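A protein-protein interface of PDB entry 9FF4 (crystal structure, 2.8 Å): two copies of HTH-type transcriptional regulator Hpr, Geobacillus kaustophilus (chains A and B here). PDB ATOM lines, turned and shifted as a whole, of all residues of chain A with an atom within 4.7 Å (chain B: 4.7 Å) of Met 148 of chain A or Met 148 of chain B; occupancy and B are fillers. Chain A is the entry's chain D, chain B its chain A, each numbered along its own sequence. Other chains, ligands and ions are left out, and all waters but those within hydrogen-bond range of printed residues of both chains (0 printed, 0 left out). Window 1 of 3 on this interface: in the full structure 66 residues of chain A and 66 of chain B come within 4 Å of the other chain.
Of the 11 printed residues of chain A, 8 touch a printed residue of chain B. Printed residues of chain A that touch a printed residue of chain B: Leu 23, Ser 24, Leu 27, Ile 145, Glu 147, Met 148, Met 149 and Val 152. Hydrophobic or aromatic side chains of chain A that line the printed part of chain B: Leu 23, Leu 27, Ile 145, Met 148, Met 149 and Val 152. Printed residues of chain B that touch a printed residue of chain A: Leu 23, Ser 24, Leu 27, Ile 145, Glu 147, Met 148, Met 149 and Val 152. Among the printed residues, 16 pairs touch across the chains.
Of chain A, only Leu 23 (3.8 Å), Leu 27 (3.7 Å), Ile 145 (3.9 Å) and Met 148 (3.4 Å) come within 4 Å of Met 148 of chain B. Of the printed residues of chain A, Val 152 of chain B touches Leu 23. Of the printed residues of chain A, Glu 147 of chain B touches Ile 145. Printed residues of chain B within 4 Å of Glu 147 of chain A: Ile 145. Ile 151 of chain A touches none of the printed residues of chain B. Leu 146 of chain B touches none of the printed residues of chain A. The nearest residue of chain B that does not touch Met 148 of chain A is Ser 24 of chain B (4.6 Å). The nearest residue of chain A that does not touch Met 148 of chain B is Ser 24 of chain A (4.6 Å). The nearest printed residue of chain B that does not touch Met 149 of chain A is Ile 145 of chain B (7.4 Å).
Leu 23 of chain A touches Ile 145 of chain B, and with the chains exchanged Ile 145 of chain A touches Leu 23 of chain B. Leu 23 of chain A touches Met 149 of chain B, and with the chains exchanged Met 149 of chain A touches Leu 23 of chain B. Leu 23 of chain A touches Val 152 of chain B, and with the chains exchanged Val 152 of chain A touches Leu 23 of chain B. Met 148 of chain A touches its own counterpart, Met 148 of chain B. 11 positions are printed for both chains.
The side-chain carboxylate of Glu 147 of chain A lies within hydrogen-bond range of the backbone NH of Ile 145 of chain B, at 2.7 Å. OE2 of Glu 147 of chain B sits at hydrogen-bond distance from N of Ile 145 of chain A (2.9 Å).
Leu 23 of chain A touches Ile 145 of chain B (CD1 to CD1, 3.7 Å). Leu 23 of chain A touches Met 148 of chain B. Leu 23 of chain A touches Met 149 of chain B. Ser 24 of chain A touches Leu 27 of chain B. CD2 of Leu 27 of chain A touches CB of Ser 24 of chain B, at 3.6 Å. N of Met 148 of chain B touches CG2 of Ile 145 of chain A, 3.9 Å away. Met 148 of chain A touches Leu 23 of chain B (SD to CB, 3.7 Å). SD of Met 148 of chain B touches CE of Met 148 of chain A, at 3.4 Å. Leu 23 of chain B touches Met 149 of chain A (CD1 to SD, 3.5 Å). CG2 of Val 152 of chain A touches CD2 of Leu 23 of chain B (3.6 Å).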
ATOM      1  N   LEU A  23     -29.159  -0.323  13.032  1.00  0.00           N
ATOM      2  CA  LEU A  23     -27.971   0.078  12.275  1.00  0.00           C
ATOM      3  C   LEU A  23     -27.826  -0.749  11.006  1.00  0.00           C
ATOM      4  O   LEU A  23     -27.698  -0.187   9.914  1.00  0.00           O
ATOM      5  CB  LEU A  23     -26.720  -0.068  13.125  1.00  0.00           C
ATOM      6  CG  LEU A  23     -26.437   1.129  14.006  1.00  0.00           C
ATOM      7  CD1 LEU A  23     -25.319   0.758  14.958  1.00  0.00           C
ATOM      8  CD2 LEU A  23     -26.061   2.336  13.152  1.00  0.00           C
ATOM      9  N   SER A  24     -27.840  -2.090  11.142  1.00  0.00           N
ATOM     10  CA  SER A  24     -27.745  -3.010  10.007  1.00  0.00           C
ATOM     11  C   SER A  24     -28.727  -2.666   8.909  1.00  0.00           C
ATOM     12  O   SER A  24     -28.395  -2.773   7.725  1.00  0.00           O
ATOM     13  CB  SER A  24     -28.023  -4.455  10.457  1.00  0.00           C
ATOM     14  OG  SER A  24     -26.866  -5.119  10.901  1.00  0.00           O
ATOM     15  N   LEU A  27     -27.789   0.719   7.362  1.00  0.00           N
ATOM     16  CA  LEU A  27     -26.585   0.629   6.548  1.00  0.00           C
ATOM     17  C   LEU A  27     -26.816  -0.206   5.289  1.00  0.00           C
ATOM     18  O   LEU A  27     -26.384   0.184   4.197  1.00  0.00           O
ATOM     19  CB  LEU A  27     -25.436   0.074   7.370  1.00  0.00           C
ATOM     20  CG  LEU A  27     -24.046   0.188   6.773  1.00  0.00           C
ATOM     21  CD1 LEU A  27     -23.477   1.630   6.719  1.00  0.00           C
ATOM     22  CD2 LEU A  27     -23.167  -0.727   7.608  1.00  0.00           C
ATOM     23  N   ILE A 145     -14.237  -0.603  11.031  1.00  0.00           N
ATOM     24  CA  ILE A 145     -15.247  -1.205  11.917  1.00  0.00           C
ATOM     25  C   ILE A 145     -14.895  -2.618  12.366  1.00  0.00           C
ATOM     26  O   ILE A 145     -15.596  -3.571  12.021  1.00  0.00           O
ATOM     27  CB  ILE A 145     -16.652  -1.179  11.276  1.00  0.00           C
ATOM     28  CG1 ILE A 145     -16.619  -1.445   9.777  1.00  0.00           C
ATOM     29  CG2 ILE A 145     -17.323   0.147  11.459  1.00  0.00           C
ATOM     30  CD1 ILE A 145     -16.143  -2.756   9.435  1.00  0.00           C
ATOM     31  N   LEU A 146     -13.816  -2.753  13.142  1.00  0.00           N
ATOM     32  CA  LEU A 146     -13.347  -4.064  13.596  1.00  0.00           C
ATOM     33  C   LEU A 146     -14.447  -4.851  14.318  1.00  0.00           C
ATOM     34  O   LEU A 146     -14.618  -6.051  14.090  1.00  0.00           O
ATOM     35  CB  LEU A 146     -12.161  -3.863  14.520  1.00  0.00           C
ATOM     36  CG  LEU A 146     -11.120  -4.938  14.613  1.00  0.00           C
ATOM     37  CD1 LEU A 146     -10.099  -4.415  15.608  1.00  0.00           C
ATOM     38  CD2 LEU A 146     -11.756  -6.253  15.029  1.00  0.00           C
ATOM     39  N   GLU A 147     -15.221  -4.183  15.172  1.00  0.00           N
ATOM     40  CA  GLU A 147     -16.262  -4.864  15.935  1.00  0.00           C
ATOM     41  C   GLU A 147     -17.218  -5.629  15.031  1.00  0.00           C
ATOM     42  O   GLU A 147     -17.631  -6.749  15.361  1.00  0.00           O
ATOM     43  CB  GLU A 147     -17.003  -3.840  16.791  1.00  0.00           C
ATOM     44  CG  GLU A 147     -16.037  -3.249  17.799  1.00  0.00           C
ATOM     45  CD  GLU A 147     -16.628  -2.201  18.713  1.00  0.00           C
ATOM     46  OE1 GLU A 147     -16.055  -2.000  19.808  1.00  0.00           O
ATOM     47  OE2 GLU A 147     -17.640  -1.559  18.338  1.00  0.00           O
ATOM     48  N   MET A 148     -17.564  -5.053  13.870  1.00  0.00           N
ATOM     49  CA  MET A 148     -18.457  -5.736  12.933  1.00  0.00           C
ATOM     50  C   MET A 148     -17.735  -6.871  12.215  1.00  0.00           C
ATOM     51  O   MET A 148     -18.336  -7.908  11.911  1.00  0.00           O
ATOM     52  CB  MET A 148     -19.009  -4.743  11.926  1.00  0.00           C
ATOM     53  CG  MET A 148     -20.428  -4.979  11.467  1.00  0.00           C
ATOM     54  SD  MET A 148     -20.563  -4.383   9.738  1.00  0.00           S
ATOM     55  CE  MET A 148     -20.217  -2.630   9.906  1.00  0.00           C
ATOM     56  N   MET A 149     -16.445  -6.699  11.941  1.00  0.00           N
ATOM     57  CA  MET A 149     -15.677  -7.803  11.387  1.00  0.00           C
ATOM     58  C   MET A 149     -15.588  -8.959  12.387  1.00  0.00           C
ATOM     59  O   MET A 149     -15.813 -10.118  12.021  1.00  0.00           O
ATOM     60  CB  MET A 149     -14.289  -7.315  10.960  1.00  0.00           C
ATOM     61  CG  MET A 149     -14.293  -6.266   9.807  1.00  0.00           C
ATOM     62  SD  MET A 149     -14.218  -6.978   8.129  1.00  0.00           S
ATOM     63  CE  MET A 149     -12.456  -7.287   7.935  1.00  0.00           C
ATOM     64  N   CYS A 150     -15.293  -8.662  13.659  1.00  0.00           N
ATOM     65  CA  CYS A 150     -15.314  -9.693  14.696  1.00  0.00           C
ATOM     66  C   CYS A 150     -16.643 -10.435  14.718  1.00  0.00           C
ATOM     67  O   CYS A 150     -16.681 -11.676  14.705  1.00  0.00           O
ATOM     68  CB  CYS A 150     -15.077  -9.073  16.066  1.00  0.00           C
ATOM     69  SG  CYS A 150     -13.429  -8.429  16.324  1.00  0.00           S
ATOM     70  N   ILE A 151     -17.747  -9.692  14.763  1.00  0.00           N
ATOM     71  CA  ILE A 151     -19.055 -10.326  14.843  1.00  0.00           C
ATOM     72  C   ILE A 151     -19.305 -11.194  13.609  1.00  0.00           C
ATOM     73  O   ILE A 151     -19.736 -12.352  13.720  1.00  0.00           O
ATOM     74  CB  ILE A 151     -20.132  -9.248  15.030  1.00  0.00           C
ATOM     75  CG1 ILE A 151     -19.907  -8.534  16.351  1.00  0.00           C
ATOM     76  CG2 ILE A 151     -21.508  -9.836  15.014  1.00  0.00           C
ATOM     77  CD1 ILE A 151     -20.846  -7.375  16.558  1.00  0.00           C
ATOM     78  N   VAL A 152     -19.008 -10.665  12.419  1.00  0.00           N
ATOM     79  CA  VAL A 152     -19.320 -11.390  11.192  1.00  0.00           C
ATOM     80  C   VAL A 152     -18.436 -12.632  11.059  1.00  0.00           C
ATOM     81  O   VAL A 152     -18.894 -13.693  10.614  1.00  0.00           O
ATOM     82  CB  VAL A 152     -19.227 -10.423   9.990  1.00  0.00           C
ATOM     83  CG1 VAL A 152     -18.992 -11.135   8.680  1.00  0.00           C
ATOM     84  CG2 VAL A 152     -20.496  -9.641   9.921  1.00  0.00           C
ATOM     85  N   LEU B  23     -19.773  -6.587   4.371  1.00  0.00           N
ATOM     86  CA  LEU B  23     -20.103  -6.633   5.786  1.00  0.00           C
ATOM     87  C   LEU B  23     -21.572  -6.324   6.005  1.00  0.00           C
ATOM     88  O   LEU B  23     -22.271  -7.076   6.694  1.00  0.00           O
ATOM     89  CB  LEU B  23     -19.248  -5.662   6.570  1.00  0.00           C
ATOM     90  CG  LEU B  23     -17.985  -6.285   7.112  1.00  0.00           C
ATOM     91  CD1 LEU B  23     -17.183  -5.176   7.667  1.00  0.00           C
ATOM     92  CD2 LEU B  23     -18.278  -7.339   8.189  1.00  0.00           C
ATOM     93  N   SER B  24     -22.076  -5.229   5.434  1.00  0.00           N
ATOM     94  CA  SER B  24     -23.429  -4.861   5.820  1.00  0.00           C
ATOM     95  C   SER B  24     -24.424  -5.875   5.286  1.00  0.00           C
ATOM     96  O   SER B  24     -25.481  -6.087   5.892  1.00  0.00           O
ATOM     97  CB  SER B  24     -23.776  -3.430   5.358  1.00  0.00           C
ATOM     98  OG  SER B  24     -23.514  -3.188   3.991  1.00  0.00           O
ATOM     99  N   LEU B  27     -24.047  -8.880   7.852  1.00  0.00           N
ATOM    100  CA  LEU B  27     -24.756  -8.511   9.062  1.00  0.00           C
ATOM    101  C   LEU B  27     -26.267  -8.495   8.833  1.00  0.00           C
ATOM    102  O   LEU B  27     -27.001  -9.239   9.488  1.00  0.00           O
ATOM    103  CB  LEU B  27     -24.246  -7.170   9.551  1.00  0.00           C
ATOM    104  CG  LEU B  27     -24.524  -6.969  11.020  1.00  0.00           C
ATOM    105  CD1 LEU B  27     -23.953  -8.097  11.879  1.00  0.00           C
ATOM    106  CD2 LEU B  27     -23.869  -5.661  11.295  1.00  0.00           C
ATOM    107  N   ILE B 145     -20.060  -0.286  18.495  1.00  0.00           N
ATOM    108  CA  ILE B 145     -20.075  -0.115  17.038  1.00  0.00           C
ATOM    109  C   ILE B 145     -20.256   1.356  16.667  1.00  0.00           C
ATOM    110  O   ILE B 145     -21.200   1.731  15.964  1.00  0.00           O
ATOM    111  CB  ILE B 145     -21.159  -0.986  16.381  1.00  0.00           C
ATOM    112  CG1 ILE B 145     -22.464  -0.911  17.170  1.00  0.00           C
ATOM    113  CG2 ILE B 145     -20.695  -2.421  16.259  1.00  0.00           C
ATOM    114  CD1 ILE B 145     -23.481  -1.919  16.726  1.00  0.00           C
ATOM    115  N   LEU B 146     -19.362   2.200  17.170  1.00  0.00           N
ATOM    116  CA  LEU B 146     -19.505   3.635  17.000  1.00  0.00           C
ATOM    117  C   LEU B 146     -19.244   4.058  15.560  1.00  0.00           C
ATOM    118  O   LEU B 146     -19.928   4.945  15.022  1.00  0.00           O
ATOM    119  CB  LEU B 146     -18.541   4.344  17.934  1.00  0.00           C
ATOM    120  CG  LEU B 146     -18.627   5.847  18.042  1.00  0.00           C
ATOM    121  CD1 LEU B 146     -20.072   6.312  18.197  1.00  0.00           C
ATOM    122  CD2 LEU B 146     -17.784   6.256  19.214  1.00  0.00           C
ATOM    123  N   GLU B 147     -18.254   3.442  14.918  1.00  0.00           N
ATOM    124  CA  GLU B 147     -17.901   3.851  13.571  1.00  0.00           C
ATOM    125  C   GLU B 147     -19.084   3.715  12.624  1.00  0.00           C
ATOM    126  O   GLU B 147     -19.268   4.559  11.738  1.00  0.00           O
ATOM    127  CB  GLU B 147     -16.697   3.054  13.083  1.00  0.00           C
ATOM    128  CG  GLU B 147     -15.412   3.570  13.693  1.00  0.00           C
ATOM    129  CD  GLU B 147     -14.167   2.806  13.266  1.00  0.00           C
ATOM    130  OE1 GLU B 147     -13.054   3.352  13.442  1.00  0.00           O
ATOM    131  OE2 GLU B 147     -14.292   1.652  12.787  1.00  0.00           O
ATOM    132  N   MET B 148     -19.928   2.693  12.802  1.00  0.00           N
ATOM    133  CA  MET B 148     -21.091   2.657  11.923  1.00  0.00           C
ATOM    134  C   MET B 148     -22.190   3.571  12.435  1.00  0.00           C
ATOM    135  O   MET B 148     -22.995   4.076  11.644  1.00  0.00           O
ATOM    136  CB  MET B 148     -21.629   1.243  11.716  1.00  0.00           C
ATOM    137  CG  MET B 148     -21.752   0.407  12.941  1.00  0.00           C
ATOM    138  SD  MET B 148     -22.056  -1.337  12.517  1.00  0.00           S
ATOM    139  CE  MET B 148     -23.359  -1.199  11.309  1.00  0.00           C
ATOM    140  N   MET B 149     -22.222   3.839  13.741  1.00  0.00           N
ATOM    141  CA  MET B 149     -23.176   4.827  14.236  1.00  0.00           C
ATOM    142  C   MET B 149     -22.878   6.207  13.645  1.00  0.00           C
ATOM    143  O   MET B 149     -23.796   6.925  13.226  1.00  0.00           O
ATOM    144  CB  MET B 149     -23.171   4.871  15.770  1.00  0.00           C
ATOM    145  CG  MET B 149     -23.751   3.624  16.445  1.00  0.00           C
ATOM    146  SD  MET B 149     -25.550   3.645  16.668  1.00  0.00           S
ATOM    147  CE  MET B 149     -25.689   4.728  18.087  1.00  0.00           C
ATOM    148  N   CYS B 150     -21.596   6.572  13.551  1.00  0.00           N
ATOM    149  CA  CYS B 150     -21.240   7.847  12.930  1.00  0.00           C
ATOM    150  C   CYS B 150     -21.598   7.850  11.460  1.00  0.00           C
ATOM    151  O   CYS B 150     -22.103   8.850  10.935  1.00  0.00           O
ATOM    152  CB  CYS B 150     -19.750   8.122  13.063  1.00  0.00           C
ATOM    153  SG  CYS B 150     -19.189   8.159  14.739  1.00  0.00           S
ATOM    154  N   ILE B 151     -21.312   6.742  10.774  1.00  0.00           N
ATOM    155  CA  ILE B 151     -21.631   6.661   9.360  1.00  0.00           C
ATOM    156  C   ILE B 151     -23.137   6.727   9.163  1.00  0.00           C
ATOM    157  O   ILE B 151     -23.631   7.484   8.320  1.00  0.00           O
ATOM    158  CB  ILE B 151     -21.028   5.388   8.738  1.00  0.00           C
ATOM    159  CG1 ILE B 151     -19.495   5.442   8.763  1.00  0.00           C
ATOM    160  CG2 ILE B 151     -21.551   5.196   7.326  1.00  0.00           C
ATOM    161  CD1 ILE B 151     -18.819   4.216   8.163  1.00  0.00           C
ATOM    162  N   VAL B 152     -23.901   5.967   9.954  1.00  0.00           N
ATOM    163  CA  VAL B 152     -25.336   5.939   9.705  1.00  0.00           C
ATOM    164  C   VAL B 152     -25.950   7.317   9.953  1.00  0.00           C
ATOM    165  O   VAL B 152     -26.846   7.749   9.213  1.00  0.00           O
ATOM    166  CB  VAL B 152     -25.999   4.818  10.518  1.00  0.00           C
ATOM    167  CG1 VAL B 152     -27.493   4.992  10.627  1.00  0.00           C
ATOM    168  CG2 VAL B 152     -25.692   3.508   9.837  1.00  0.00           C
